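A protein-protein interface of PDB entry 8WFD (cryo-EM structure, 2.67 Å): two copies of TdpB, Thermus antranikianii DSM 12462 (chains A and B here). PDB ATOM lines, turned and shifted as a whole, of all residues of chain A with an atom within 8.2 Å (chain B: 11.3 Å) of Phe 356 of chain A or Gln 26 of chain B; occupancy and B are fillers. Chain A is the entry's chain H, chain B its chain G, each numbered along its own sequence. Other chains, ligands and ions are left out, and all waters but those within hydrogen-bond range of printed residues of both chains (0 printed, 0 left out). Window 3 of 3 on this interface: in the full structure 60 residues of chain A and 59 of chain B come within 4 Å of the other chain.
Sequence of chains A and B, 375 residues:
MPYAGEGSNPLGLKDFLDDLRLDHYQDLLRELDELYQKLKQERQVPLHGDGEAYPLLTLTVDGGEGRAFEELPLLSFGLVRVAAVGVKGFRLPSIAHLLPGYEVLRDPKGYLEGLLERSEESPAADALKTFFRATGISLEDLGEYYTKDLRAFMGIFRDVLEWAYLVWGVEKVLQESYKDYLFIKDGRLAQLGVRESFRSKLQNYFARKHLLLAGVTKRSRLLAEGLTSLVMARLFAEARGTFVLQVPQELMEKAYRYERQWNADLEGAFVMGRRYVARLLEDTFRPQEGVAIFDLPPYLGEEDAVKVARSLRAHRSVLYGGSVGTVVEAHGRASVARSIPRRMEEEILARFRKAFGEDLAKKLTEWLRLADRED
No position is printed for both chains.
OH of Tyr 102 of chain A lies within hydrogen-bond range of OD2 of Asp 27 of chain B, 2.8 Å away.
The side-chain hydroxyl (OH) of Tyr 102 of chain A is in hydrogen-bond range of the side-chain carboxylate (OE2) of Glu 31 of chain B, 2.6 Å away.
Ile 348 of chain A touches Leu 20 of chain B.
Leu 22 of chain B touches Ile 348 of chain A.
Ile 348 of chain A touches Tyr 25 of chain B.
CD of Arg 351 of chain A touches CD1 of Leu 20 of chain B (3.6 Å).
N of Phe 352 of chain A touches CD1 of Leu 22 of chain B, at 3.5 Å.
CE1 of Phe 352 of chain A touches CB of Tyr 25 of chain B (3.7 Å).
Phe 352 of chain A touches Leu 29 of chain B.
O of Leu 22 of chain B touches CZ of Phe 356 of chain A, at 2.9 Å.
Phe 356 of chain A touches Gln 26 of chain B.
Leu 360 of chain A touches Leu 29 of chain B (CD1 to CD1, 3.4 Å).
OE1 of Glu 31 of chain B lies within hydrogen-bond range of OH of Tyr 258 of chain B (2.4 Å).
Phe 356 of chain A touches just these residues of chain B: Leu 22 and Gln 26.
Printed residues of chain A within 4 Å of Gln 26 of chain B: Phe 356.
No residue of chain B comes within 4 Å of Ala 355 of chain A.
Of chain B, only Leu 29 comes within 4 Å of Leu 360 of chain A.
Of the printed residues of chain A, Asp 33 of chain B touches Lys 363.
Of the printed residues of chain A, Tyr 25 of chain B touches Ile 348 and Phe 352.
Of the printed residues of chain B, Ile 348 of chain A touches Leu 20, Leu 22 and Tyr 25.
Printed residues of chain B within 4 Å of Tyr 102 of chain A: His 24 (3.6 Å), Asp 27 (2.8 Å) and Glu 31 (2.6 Å).
Printed residues of chain A within 4 Å of Leu 20 of chain B: Ile 348 (3.5 Å) and Arg 351 (3.6 Å).
Asp 359 of chain A touches none of the printed residues of chain B.
Arg 21 of chain B touches none of the printed residues of chain A.
The nearest residue of chain B that does not touch Phe 356 of chain A is Asp 23 of chain B (4.9 Å).
The nearest residue of chain A that does not touch Gln 26 of chain B is Phe 352 of chain A (4.2 Å).
The nearest printed residue of chain A that does not touch Leu 22 of chain B is Ala 355 of chain A (4.4 Å).
Hydrophobic or aromatic side chains of chain B that line the printed part of chain A: Leu 20, Leu 22, His 24, Tyr 25 and Leu 29.
Of the 18 printed residues of chain A, 8 touch a printed residue of chain B.
Hydrophobic or aromatic side chains of chain A that line the printed part of chain B: Tyr 102, Ile 348, Phe 352, Phe 356, Leu 360 and Leu 364.
Among the printed residues, no Asp or Glu carboxylate lies within 4 Å of a Lys or Arg side-chain nitrogen of the other chain.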
ATOM      1  N   TYR A 102      30.326   8.954 -16.962  1.00  0.00           N
ATOM      2  CA  TYR A 102      29.285   9.901 -16.583  1.00  0.00           C
ATOM      3  C   TYR A 102      29.742  11.334 -16.826  1.00  0.00           C
ATOM      4  O   TYR A 102      29.183  12.026 -17.683  1.00  0.00           O
ATOM      5  CB  TYR A 102      28.895   9.705 -15.117  1.00  0.00           C
ATOM      6  CG  TYR A 102      27.695  10.514 -14.685  1.00  0.00           C
ATOM      7  CD1 TYR A 102      26.406  10.080 -14.966  1.00  0.00           C
ATOM      8  CD2 TYR A 102      27.848  11.705 -13.989  1.00  0.00           C
ATOM      9  CE1 TYR A 102      25.305  10.812 -14.571  1.00  0.00           C
ATOM     10  CE2 TYR A 102      26.751  12.444 -13.589  1.00  0.00           C
ATOM     11  CZ  TYR A 102      25.482  11.993 -13.883  1.00  0.00           C
ATOM     12  OH  TYR A 102      24.384  12.724 -13.489  1.00  0.00           O
ATOM     13  N   ILE A 348      39.500   3.325  -7.598  1.00  0.00           N
ATOM     14  CA  ILE A 348      38.543   4.424  -7.586  1.00  0.00           C
ATOM     15  C   ILE A 348      37.544   4.240  -6.454  1.00  0.00           C
ATOM     16  O   ILE A 348      37.178   5.202  -5.770  1.00  0.00           O
ATOM     17  CB  ILE A 348      37.843   4.539  -8.952  1.00  0.00           C
ATOM     18  CG1 ILE A 348      38.858   4.901 -10.038  1.00  0.00           C
ATOM     19  CG2 ILE A 348      36.730   5.572  -8.893  1.00  0.00           C
ATOM     20  CD1 ILE A 348      38.283   4.911 -11.434  1.00  0.00           C
ATOM     21  N   LEU A 349      37.084   3.004  -6.237  1.00  0.00           N
ATOM     22  CA  LEU A 349      36.192   2.749  -5.111  1.00  0.00           C
ATOM     23  C   LEU A 349      36.859   3.076  -3.781  1.00  0.00           C
ATOM     24  O   LEU A 349      36.232   3.682  -2.907  1.00  0.00           O
ATOM     25  CB  LEU A 349      35.731   1.293  -5.123  1.00  0.00           C
ATOM     26  CG  LEU A 349      34.658   0.920  -6.145  1.00  0.00           C
ATOM     27  CD1 LEU A 349      34.539  -0.590  -6.255  1.00  0.00           C
ATOM     28  CD2 LEU A 349      33.324   1.542  -5.769  1.00  0.00           C
ATOM     29  N   ALA A 350      38.123   2.682  -3.611  1.00  0.00           N
ATOM     30  CA  ALA A 350      38.826   2.967  -2.363  1.00  0.00           C
ATOM     31  C   ALA A 350      38.977   4.469  -2.142  1.00  0.00           C
ATOM     32  O   ALA A 350      38.757   4.971  -1.032  1.00  0.00           O
ATOM     33  CB  ALA A 350      40.192   2.282  -2.363  1.00  0.00           C
ATOM     34  N   ARG A 351      39.363   5.203  -3.189  1.00  0.00           N
ATOM     35  CA  ARG A 351      39.508   6.649  -3.053  1.00  0.00           C
ATOM     36  C   ARG A 351      38.174   7.321  -2.768  1.00  0.00           C
ATOM     37  O   ARG A 351      38.114   8.263  -1.971  1.00  0.00           O
ATOM     38  CB  ARG A 351      40.151   7.243  -4.306  1.00  0.00           C
ATOM     39  CG  ARG A 351      41.573   6.777  -4.554  1.00  0.00           C
ATOM     40  CD  ARG A 351      42.234   7.594  -5.650  1.00  0.00           C
ATOM     41  NE  ARG A 351      43.538   7.057  -6.019  1.00  0.00           N
ATOM     42  CZ  ARG A 351      44.668   7.329  -5.380  1.00  0.00           C
ATOM     43  NH1 ARG A 351      44.691   8.132  -4.328  1.00  0.00           N
ATOM     44  NH2 ARG A 351      45.802   6.781  -5.806  1.00  0.00           N
ATOM     45  N   PHE A 352      37.097   6.862  -3.408  1.00  0.00           N
ATOM     46  CA  PHE A 352      35.774   7.392  -3.096  1.00  0.00           C
ATOM     47  C   PHE A 352      35.415   7.136  -1.639  1.00  0.00           C
ATOM     48  O   PHE A 352      34.882   8.018  -0.957  1.00  0.00           O
ATOM     49  CB  PHE A 352      34.732   6.771  -4.025  1.00  0.00           C
ATOM     50  CG  PHE A 352      33.391   7.440  -3.969  1.00  0.00           C
ATOM     51  CD1 PHE A 352      33.213   8.708  -4.492  1.00  0.00           C
ATOM     52  CD2 PHE A 352      32.308   6.799  -3.396  1.00  0.00           C
ATOM     53  CE1 PHE A 352      31.980   9.325  -4.442  1.00  0.00           C
ATOM     54  CE2 PHE A 352      31.074   7.411  -3.344  1.00  0.00           C
ATOM     55  CZ  PHE A 352      30.910   8.676  -3.867  1.00  0.00           C
ATOM     56  N   ARG A 353      35.711   5.933  -1.143  1.00  0.00           N
ATOM     57  CA  ARG A 353      35.419   5.619   0.250  1.00  0.00           C
ATOM     58  C   ARG A 353      36.189   6.530   1.194  1.00  0.00           C
ATOM     59  O   ARG A 353      35.632   7.024   2.182  1.00  0.00           O
ATOM     60  CB  ARG A 353      35.753   4.156   0.543  1.00  0.00           C
ATOM     61  CG  ARG A 353      35.406   3.719   1.956  1.00  0.00           C
ATOM     62  CD  ARG A 353      35.795   2.274   2.196  1.00  0.00           C
ATOM     63  NE  ARG A 353      35.061   1.358   1.332  1.00  0.00           N
ATOM     64  CZ  ARG A 353      35.606   0.671   0.339  1.00  0.00           C
ATOM     65  NH1 ARG A 353      36.893   0.777   0.049  1.00  0.00           N
ATOM     66  NH2 ARG A 353      34.841  -0.144  -0.384  1.00  0.00           N
ATOM     67  N   LYS A 354      37.468   6.764   0.914  1.00  0.00           N
ATOM     68  CA  LYS A 354      38.301   7.552   1.814  1.00  0.00           C
ATOM     69  C   LYS A 354      38.140   9.055   1.621  1.00  0.00           C
ATOM     70  O   LYS A 354      38.640   9.825   2.447  1.00  0.00           O
ATOM     71  CB  LYS A 354      39.776   7.166   1.658  1.00  0.00           C
ATOM     72  CG  LYS A 354      40.427   7.621   0.365  1.00  0.00           C
ATOM     73  CD  LYS A 354      41.820   7.021   0.227  1.00  0.00           C
ATOM     74  CE  LYS A 354      42.573   7.625  -0.946  1.00  0.00           C
ATOM     75  NZ  LYS A 354      43.006   9.019  -0.660  1.00  0.00           N
ATOM     76  N   ALA A 355      37.459   9.492   0.559  1.00  0.00           N
ATOM     77  CA  ALA A 355      37.188  10.908   0.357  1.00  0.00           C
ATOM     78  C   ALA A 355      35.748  11.304   0.649  1.00  0.00           C
ATOM     79  O   ALA A 355      35.467  12.502   0.749  1.00  0.00           O
ATOM     80  CB  ALA A 355      37.533  11.318  -1.082  1.00  0.00           C
ATOM     81  N   PHE A 356      34.840  10.340   0.782  1.00  0.00           N
ATOM     82  CA  PHE A 356      33.451  10.595   1.143  1.00  0.00           C
ATOM     83  C   PHE A 356      33.025   9.600   2.217  1.00  0.00           C
ATOM     84  O   PHE A 356      33.841   8.855   2.767  1.00  0.00           O
ATOM     85  CB  PHE A 356      32.530  10.513  -0.080  1.00  0.00           C
ATOM     86  CG  PHE A 356      32.923  11.435  -1.198  1.00  0.00           C
ATOM     87  CD1 PHE A 356      32.418  12.721  -1.262  1.00  0.00           C
ATOM     88  CD2 PHE A 356      33.798  11.015  -2.184  1.00  0.00           C
ATOM     89  CE1 PHE A 356      32.777  13.572  -2.285  1.00  0.00           C
ATOM     90  CE2 PHE A 356      34.161  11.861  -3.213  1.00  0.00           C
ATOM     91  CZ  PHE A 356      33.650  13.142  -3.262  1.00  0.00           C
ATOM     92  N   GLY A 357      31.730   9.591   2.517  1.00  0.00           N
ATOM     93  CA  GLY A 357      31.234   8.752   3.588  1.00  0.00           C
ATOM     94  C   GLY A 357      31.227   7.280   3.221  1.00  0.00           C
ATOM     95  O   GLY A 357      31.046   6.893   2.063  1.00  0.00           O
ATOM     96  N   GLU A 358      31.422   6.442   4.242  1.00  0.00           N
ATOM     97  CA  GLU A 358      31.332   5.003   4.034  1.00  0.00           C
ATOM     98  C   GLU A 358      29.935   4.595   3.596  1.00  0.00           C
ATOM     99  O   GLU A 358      29.787   3.650   2.817  1.00  0.00           O
ATOM    100  CB  GLU A 358      31.736   4.255   5.304  1.00  0.00           C
ATOM    101  CG  GLU A 358      33.240   4.127   5.493  1.00  0.00           C
ATOM    102  CD  GLU A 358      33.877   5.411   5.986  1.00  0.00           C
ATOM    103  OE1 GLU A 358      33.134   6.371   6.281  1.00  0.00           O
ATOM    104  OE2 GLU A 358      35.121   5.461   6.078  1.00  0.00           O
ATOM    105  N   ASP A 359      28.902   5.292   4.074  1.00  0.00           N
ATOM    106  CA  ASP A 359      27.550   5.026   3.594  1.00  0.00           C
ATOM    107  C   ASP A 359      27.438   5.295   2.098  1.00  0.00           C
ATOM    108  O   ASP A 359      26.846   4.500   1.358  1.00  0.00           O
ATOM    109  CB  ASP A 359      26.546   5.877   4.372  1.00  0.00           C
ATOM    110  CG  ASP A 359      25.161   5.872   3.748  1.00  0.00           C
ATOM    111  OD1 ASP A 359      24.845   4.938   2.982  1.00  0.00           O
ATOM    112  OD2 ASP A 359      24.386   6.812   4.025  1.00  0.00           O
ATOM    113  N   LEU A 360      27.997   6.413   1.635  1.00  0.00           N
ATOM    114  CA  LEU A 360      27.954   6.735   0.212  1.00  0.00           C
ATOM    115  C   LEU A 360      28.713   5.697  -0.606  1.00  0.00           C
ATOM    116  O   LEU A 360      28.234   5.232  -1.652  1.00  0.00           O
ATOM    117  CB  LEU A 360      28.529   8.137  -0.007  1.00  0.00           C
ATOM    118  CG  LEU A 360      28.542   8.747  -1.405  1.00  0.00           C
ATOM    119  CD1 LEU A 360      27.124   8.917  -1.919  1.00  0.00           C
ATOM    120  CD2 LEU A 360      29.267  10.081  -1.383  1.00  0.00           C
ATOM    121  N   ALA A 361      29.902   5.311  -0.134  1.00  0.00           N
ATOM    122  CA  ALA A 361      30.685   4.303  -0.842  1.00  0.00           C
ATOM    123  C   ALA A 361      29.953   2.969  -0.886  1.00  0.00           C
ATOM    124  O   ALA A 361      29.972   2.272  -1.907  1.00  0.00           O
ATOM    125  CB  ALA A 361      32.056   4.149  -0.187  1.00  0.00           C
ATOM    126  N   LYS A 362      29.294   2.598   0.213  1.00  0.00           N
ATOM    127  CA  LYS A 362      28.559   1.340   0.259  1.00  0.00           C
ATOM    128  C   LYS A 362      27.341   1.377  -0.655  1.00  0.00           C
ATOM    129  O   LYS A 362      26.988   0.364  -1.263  1.00  0.00           O
ATOM    130  CB  LYS A 362      28.150   1.032   1.698  1.00  0.00           C
ATOM    131  CG  LYS A 362      27.571  -0.353   1.908  1.00  0.00           C
ATOM    132  CD  LYS A 362      26.058  -0.313   1.990  1.00  0.00           C
ATOM    133  CE  LYS A 362      25.508  -1.628   2.513  1.00  0.00           C
ATOM    134  NZ  LYS A 362      24.035  -1.575   2.711  1.00  0.00           N
ATOM    135  N   LYS A 363      26.681   2.530  -0.760  1.00  0.00           N
ATOM    136  CA  LYS A 363      25.567   2.657  -1.696  1.00  0.00           C
ATOM    137  C   LYS A 363      26.042   2.498  -3.136  1.00  0.00           C
ATOM    138  O   LYS A 363      25.409   1.799  -3.942  1.00  0.00           O
ATOM    139  CB  LYS A 363      24.878   4.007  -1.494  1.00  0.00           C
ATOM    140  CG  LYS A 363      23.671   4.252  -2.378  1.00  0.00           C
ATOM    141  CD  LYS A 363      22.947   5.520  -1.947  1.00  0.00           C
ATOM    142  CE  LYS A 363      21.674   5.738  -2.744  1.00  0.00           C
ATOM    143  NZ  LYS A 363      21.954   6.344  -4.072  1.00  0.00           N
ATOM    144  N   LEU A 364      27.168   3.132  -3.476  1.00  0.00           N
ATOM    145  CA  LEU A 364      27.723   2.960  -4.815  1.00  0.00           C
ATOM    146  C   LEU A 364      28.089   1.501  -5.069  1.00  0.00           C
ATOM    147  O   LEU A 364      27.831   0.963  -6.154  1.00  0.00           O
ATOM    148  CB  LEU A 364      28.939   3.868  -4.999  1.00  0.00           C
ATOM    149  CG  LEU A 364      29.823   3.616  -6.222  1.00  0.00           C
ATOM    150  CD1 LEU A 364      29.037   3.829  -7.502  1.00  0.00           C
ATOM    151  CD2 LEU A 364      31.049   4.513  -6.190  1.00  0.00           C
ATOM    152  N   LEU B  20      42.751  11.367 -10.729  1.00  0.00           N
ATOM    153  CA  LEU B  20      41.425  10.805 -10.507  1.00  0.00           C
ATOM    154  C   LEU B  20      40.485  11.863  -9.940  1.00  0.00           C
ATOM    155  O   LEU B  20      40.884  12.706  -9.130  1.00  0.00           O
ATOM    156  CB  LEU B  20      41.509   9.608  -9.560  1.00  0.00           C
ATOM    157  CG  LEU B  20      41.477   8.232 -10.226  1.00  0.00           C
ATOM    158  CD1 LEU B  20      41.465   7.127  -9.184  1.00  0.00           C
ATOM    159  CD2 LEU B  20      40.275   8.119 -11.147  1.00  0.00           C
ATOM    160  N   ARG B  21      39.229  11.819 -10.377  1.00  0.00           N
ATOM    161  CA  ARG B  21      38.206  12.772  -9.965  1.00  0.00           C
ATOM    162  C   ARG B  21      37.009  12.000  -9.427  1.00  0.00           C
ATOM    163  O   ARG B  21      36.543  11.052 -10.067  1.00  0.00           O
ATOM    164  CB  ARG B  21      37.793  13.669 -11.134  1.00  0.00           C
ATOM    165  CG  ARG B  21      38.925  14.530 -11.676  1.00  0.00           C
ATOM    166  CD  ARG B  21      38.577  15.118 -13.035  1.00  0.00           C
ATOM    167  NE  ARG B  21      37.322  15.857 -13.010  1.00  0.00           N
ATOM    168  CZ  ARG B  21      37.205  17.120 -12.624  1.00  0.00           C
ATOM    169  NH1 ARG B  21      38.253  17.820 -12.222  1.00  0.00           N
ATOM    170  NH2 ARG B  21      36.006  17.696 -12.642  1.00  0.00           N
ATOM    171  N   LEU B  22      36.515  12.402  -8.257  1.00  0.00           N
ATOM    172  CA  LEU B  22      35.441  11.664  -7.605  1.00  0.00           C
ATOM    173  C   LEU B  22      34.274  12.566  -7.215  1.00  0.00           C
ATOM    174  O   LEU B  22      33.766  12.478  -6.094  1.00  0.00           O
ATOM    175  CB  LEU B  22      35.976  10.936  -6.369  1.00  0.00           C
ATOM    176  CG  LEU B  22      37.347  10.267  -6.510  1.00  0.00           C
ATOM    177  CD1 LEU B  22      37.869   9.819  -5.152  1.00  0.00           C
ATOM    178  CD2 LEU B  22      37.286   9.094  -7.476  1.00  0.00           C
ATOM    179  N   ASP B  23      33.840  13.430  -8.129  1.00  0.00           N
ATOM    180  CA  ASP B  23      32.673  14.280  -7.919  1.00  0.00           C
ATOM    181  C   ASP B  23      31.488  13.881  -8.781  1.00  0.00           C
ATOM    182  O   ASP B  23      30.339  13.944  -8.324  1.00  0.00           O
ATOM    183  CB  ASP B  23      33.032  15.746  -8.197  1.00  0.00           C
ATOM    184  CG  ASP B  23      31.816  16.652  -8.227  1.00  0.00           C
ATOM    185  OD1 ASP B  23      30.838  16.370  -7.502  1.00  0.00           O
ATOM    186  OD2 ASP B  23      31.840  17.651  -8.977  1.00  0.00           O
ATOM    187  N   HIS B  24      31.742  13.461 -10.021  1.00  0.00           N
ATOM    188  CA  HIS B  24      30.660  12.960 -10.854  1.00  0.00           C
ATOM    189  C   HIS B  24      30.002  11.738 -10.228  1.00  0.00           C
ATOM    190  O   HIS B  24      28.827  11.475 -10.487  1.00  0.00           O
ATOM    191  CB  HIS B  24      31.175  12.632 -12.254  1.00  0.00           C
ATOM    192  CG  HIS B  24      32.187  11.530 -12.285  1.00  0.00           C
ATOM    193  ND1 HIS B  24      33.497  11.710 -11.894  1.00  0.00           N
ATOM    194  CD2 HIS B  24      32.083  10.235 -12.664  1.00  0.00           C
ATOM    195  CE1 HIS B  24      34.155  10.572 -12.029  1.00  0.00           C
ATOM    196  NE2 HIS B  24      33.319   9.661 -12.495  1.00  0.00           N
ATOM    197  N   TYR B  25      30.729  10.992  -9.395  1.00  0.00           N
ATOM    198  CA  TYR B  25      30.111   9.867  -8.700  1.00  0.00           C
ATOM    199  C   TYR B  25      29.061  10.344  -7.703  1.00  0.00           C
ATOM    200  O   TYR B  25      27.973   9.761  -7.608  1.00  0.00           O
ATOM    201  CB  TYR B  25      31.181   9.025  -8.006  1.00  0.00           C
ATOM    202  CG  TYR B  25      31.934   8.124  -8.957  1.00  0.00           C
ATOM    203  CD1 TYR B  25      31.259   7.222  -9.768  1.00  0.00           C
ATOM    204  CD2 TYR B  25      33.318   8.178  -9.049  1.00  0.00           C
ATOM    205  CE1 TYR B  25      31.939   6.398 -10.643  1.00  0.00           C
ATOM    206  CE2 TYR B  25      34.006   7.357  -9.922  1.00  0.00           C
ATOM    207  CZ  TYR B  25      33.312   6.469 -10.715  1.00  0.00           C
ATOM    208  OH  TYR B  25      33.990   5.648 -11.585  1.00  0.00           O
ATOM    209  N   GLN B  26      29.364  11.403  -6.948  1.00  0.00           N
ATOM    210  CA  GLN B  26      28.359  11.972  -6.057  1.00  0.00           C
ATOM    211  C   GLN B  26      27.201  12.562  -6.850  1.00  0.00           C
ATOM    212  O   GLN B  26      26.041  12.465  -6.434  1.00  0.00           O
ATOM    213  CB  GLN B  26      28.982  13.030  -5.148  1.00  0.00           C
ATOM    214  CG  GLN B  26      28.121  13.361  -3.936  1.00  0.00           C
ATOM    215  CD  GLN B  26      28.884  14.086  -2.847  1.00  0.00           C
ATOM    216  OE1 GLN B  26      30.056  14.422  -3.013  1.00  0.00           O
ATOM    217  NE2 GLN B  26      28.222  14.330  -1.723  1.00  0.00           N
ATOM    218  N   ASP B  27      27.498  13.184  -7.994  1.00  0.00           N
ATOM    219  CA  ASP B  27      26.426  13.681  -8.853  1.00  0.00           C
ATOM    220  C   ASP B  27      25.523  12.542  -9.313  1.00  0.00           C
ATOM    221  O   ASP B  27      24.296  12.690  -9.366  1.00  0.00           O
ATOM    222  CB  ASP B  27      27.019  14.415 -10.056  1.00  0.00           C
ATOM    223  CG  ASP B  27      25.980  15.205 -10.828  1.00  0.00           C
ATOM    224  OD1 ASP B  27      25.574  16.282 -10.345  1.00  0.00           O
ATOM    225  OD2 ASP B  27      25.571  14.752 -11.917  1.00  0.00           O
ATOM    226  N   LEU B  28      26.119  11.399  -9.652  1.00  0.00           N
ATOM    227  CA  LEU B  28      25.354  10.253 -10.129  1.00  0.00           C
ATOM    228  C   LEU B  28      24.526   9.630  -9.014  1.00  0.00           C
ATOM    229  O   LEU B  28      23.394   9.189  -9.247  1.00  0.00           O
ATOM    230  CB  LEU B  28      26.300   9.218 -10.733  1.00  0.00           C
ATOM    231  CG  LEU B  28      25.763   7.794 -10.867  1.00  0.00           C
ATOM    232  CD1 LEU B  28      24.704   7.716 -11.954  1.00  0.00           C
ATOM    233  CD2 LEU B  28      26.904   6.834 -11.145  1.00  0.00           C
ATOM    234  N   LEU B  29      25.068   9.576  -7.797  1.00  0.00           N
ATOM    235  CA  LEU B  29      24.311   8.976  -6.706  1.00  0.00           C
ATOM    236  C   LEU B  29      23.318   9.982  -6.141  1.00  0.00           C
ATOM    237  O   LEU B  29      23.217  10.156  -4.923  1.00  0.00           O
ATOM    238  CB  LEU B  29      25.243   8.487  -5.596  1.00  0.00           C
ATOM    239  CG  LEU B  29      26.299   7.439  -5.940  1.00  0.00           C
ATOM    240  CD1 LEU B  29      27.486   7.573  -5.001  1.00  0.00           C
ATOM    241  CD2 LEU B  29      25.708   6.044  -5.859  1.00  0.00           C
ATOM    242  N   ARG B  30      22.592  10.643  -7.018  1.00  0.00           N
ATOM    243  CA  ARG B  30      21.411  11.426  -6.687  1.00  0.00           C
ATOM    244  C   ARG B  30      20.249  11.120  -7.615  1.00  0.00           C
ATOM    245  O   ARG B  30      19.120  10.934  -7.148  1.00  0.00           O
ATOM    246  CB  ARG B  30      21.771  12.921  -6.740  1.00  0.00           C
ATOM    247  CG  ARG B  30      20.627  13.884  -6.482  1.00  0.00           C
ATOM    248  CD  ARG B  30      21.180  15.254  -6.110  1.00  0.00           C
ATOM    249  NE  ARG B  30      20.214  16.327  -6.317  1.00  0.00           N
ATOM    250  CZ  ARG B  30      19.236  16.627  -5.476  1.00  0.00           C
ATOM    251  NH1 ARG B  30      19.058  15.953  -4.351  1.00  0.00           N
ATOM    252  NH2 ARG B  30      18.416  17.633  -5.767  1.00  0.00           N
ATOM    253  N   GLU B  31      20.514  10.985  -8.916  1.00  0.00           N
ATOM    254  CA  GLU B  31      19.462  10.658  -9.869  1.00  0.00           C
ATOM    255  C   GLU B  31      18.998   9.220  -9.705  1.00  0.00           C
ATOM    256  O   GLU B  31      17.805   8.933  -9.836  1.00  0.00           O
ATOM    257  CB  GLU B  31      19.950  10.902 -11.298  1.00  0.00           C
ATOM    258  CG  GLU B  31      20.270  12.357 -11.606  1.00  0.00           C
ATOM    259  CD  GLU B  31      21.211  12.508 -12.782  1.00  0.00           C
ATOM    260  OE1 GLU B  31      21.179  11.645 -13.684  1.00  0.00           O
ATOM    261  OE2 GLU B  31      21.983  13.489 -12.807  1.00  0.00           O
ATOM    262  N   LEU B  32      19.924   8.303  -9.417  1.00  0.00           N
ATOM    263  CA  LEU B  32      19.534   6.917  -9.184  1.00  0.00           C
ATOM    264  C   LEU B  32      18.629   6.804  -7.964  1.00  0.00           C
ATOM    265  O   LEU B  32      17.615   6.096  -7.993  1.00  0.00           O
ATOM    266  CB  LEU B  32      20.779   6.047  -9.017  1.00  0.00           C
ATOM    267  CG  LEU B  32      21.783   6.079 -10.171  1.00  0.00           C
ATOM    268  CD1 LEU B  32      22.637   4.820 -10.179  1.00  0.00           C
ATOM    269  CD2 LEU B  32      21.073   6.258 -11.502  1.00  0.00           C
ATOM    270  N   ASP B  33      18.973   7.506  -6.881  1.00  0.00           N
ATOM    271  CA  ASP B  33      18.128   7.493  -5.692  1.00  0.00           C
ATOM    272  C   ASP B  33      16.770   8.124  -5.972  1.00  0.00           C
ATOM    273  O   ASP B  33      15.734   7.615  -5.524  1.00  0.00           O
ATOM    274  CB  ASP B  33      18.831   8.215  -4.543  1.00  0.00           C
ATOM    275  CG  ASP B  33      18.193   7.929  -3.198  1.00  0.00           C
ATOM    276  OD1 ASP B  33      17.501   6.896  -3.075  1.00  0.00           O
ATOM    277  OD2 ASP B  33      18.388   8.733  -2.264  1.00  0.00           O
ATOM    278  N   GLU B  34      16.750   9.238  -6.708  1.00  0.00           N
ATOM    279  CA  GLU B  34      15.479   9.869  -7.045  1.00  0.00           C
ATOM    280  C   GLU B  34      14.607   8.930  -7.871  1.00  0.00           C
ATOM    281  O   GLU B  34      13.399   8.816  -7.636  1.00  0.00           O
ATOM    282  CB  GLU B  34      15.727  11.180  -7.792  1.00  0.00           C
ATOM    283  CG  GLU B  34      16.372  12.261  -6.941  1.00  0.00           C
ATOM    284  CD  GLU B  34      15.585  12.557  -5.679  1.00  0.00           C
ATOM    285  OE1 GLU B  34      14.344  12.413  -5.704  1.00  0.00           O
ATOM    286  OE2 GLU B  34      16.206  12.933  -4.663  1.00  0.00           O
ATOM    287  N   TYR B 258      19.566   9.351 -22.029  1.00  0.00           N
ATOM    288  CA  TYR B 258      20.863   8.686 -21.959  1.00  0.00           C
ATOM    289  C   TYR B 258      21.150   7.896 -23.231  1.00  0.00           C
ATOM    290  O   TYR B 258      22.263   7.951 -23.769  1.00  0.00           O
ATOM    291  CB  TYR B 258      20.925   7.779 -20.729  1.00  0.00           C
ATOM    292  CG  TYR B 258      21.052   8.534 -19.425  1.00  0.00           C
ATOM    293  CD1 TYR B 258      22.045   9.486 -19.248  1.00  0.00           C
ATOM    294  CD2 TYR B 258      20.182   8.291 -18.372  1.00  0.00           C
ATOM    295  CE1 TYR B 258      22.166  10.178 -18.057  1.00  0.00           C
ATOM    296  CE2 TYR B 258      20.296   8.977 -17.177  1.00  0.00           C
ATOM    297  CZ  TYR B 258      21.289   9.920 -17.025  1.00  0.00           C
ATOM    298  OH  TYR B 258      21.406  10.606 -15.839  1.00  0.00           O
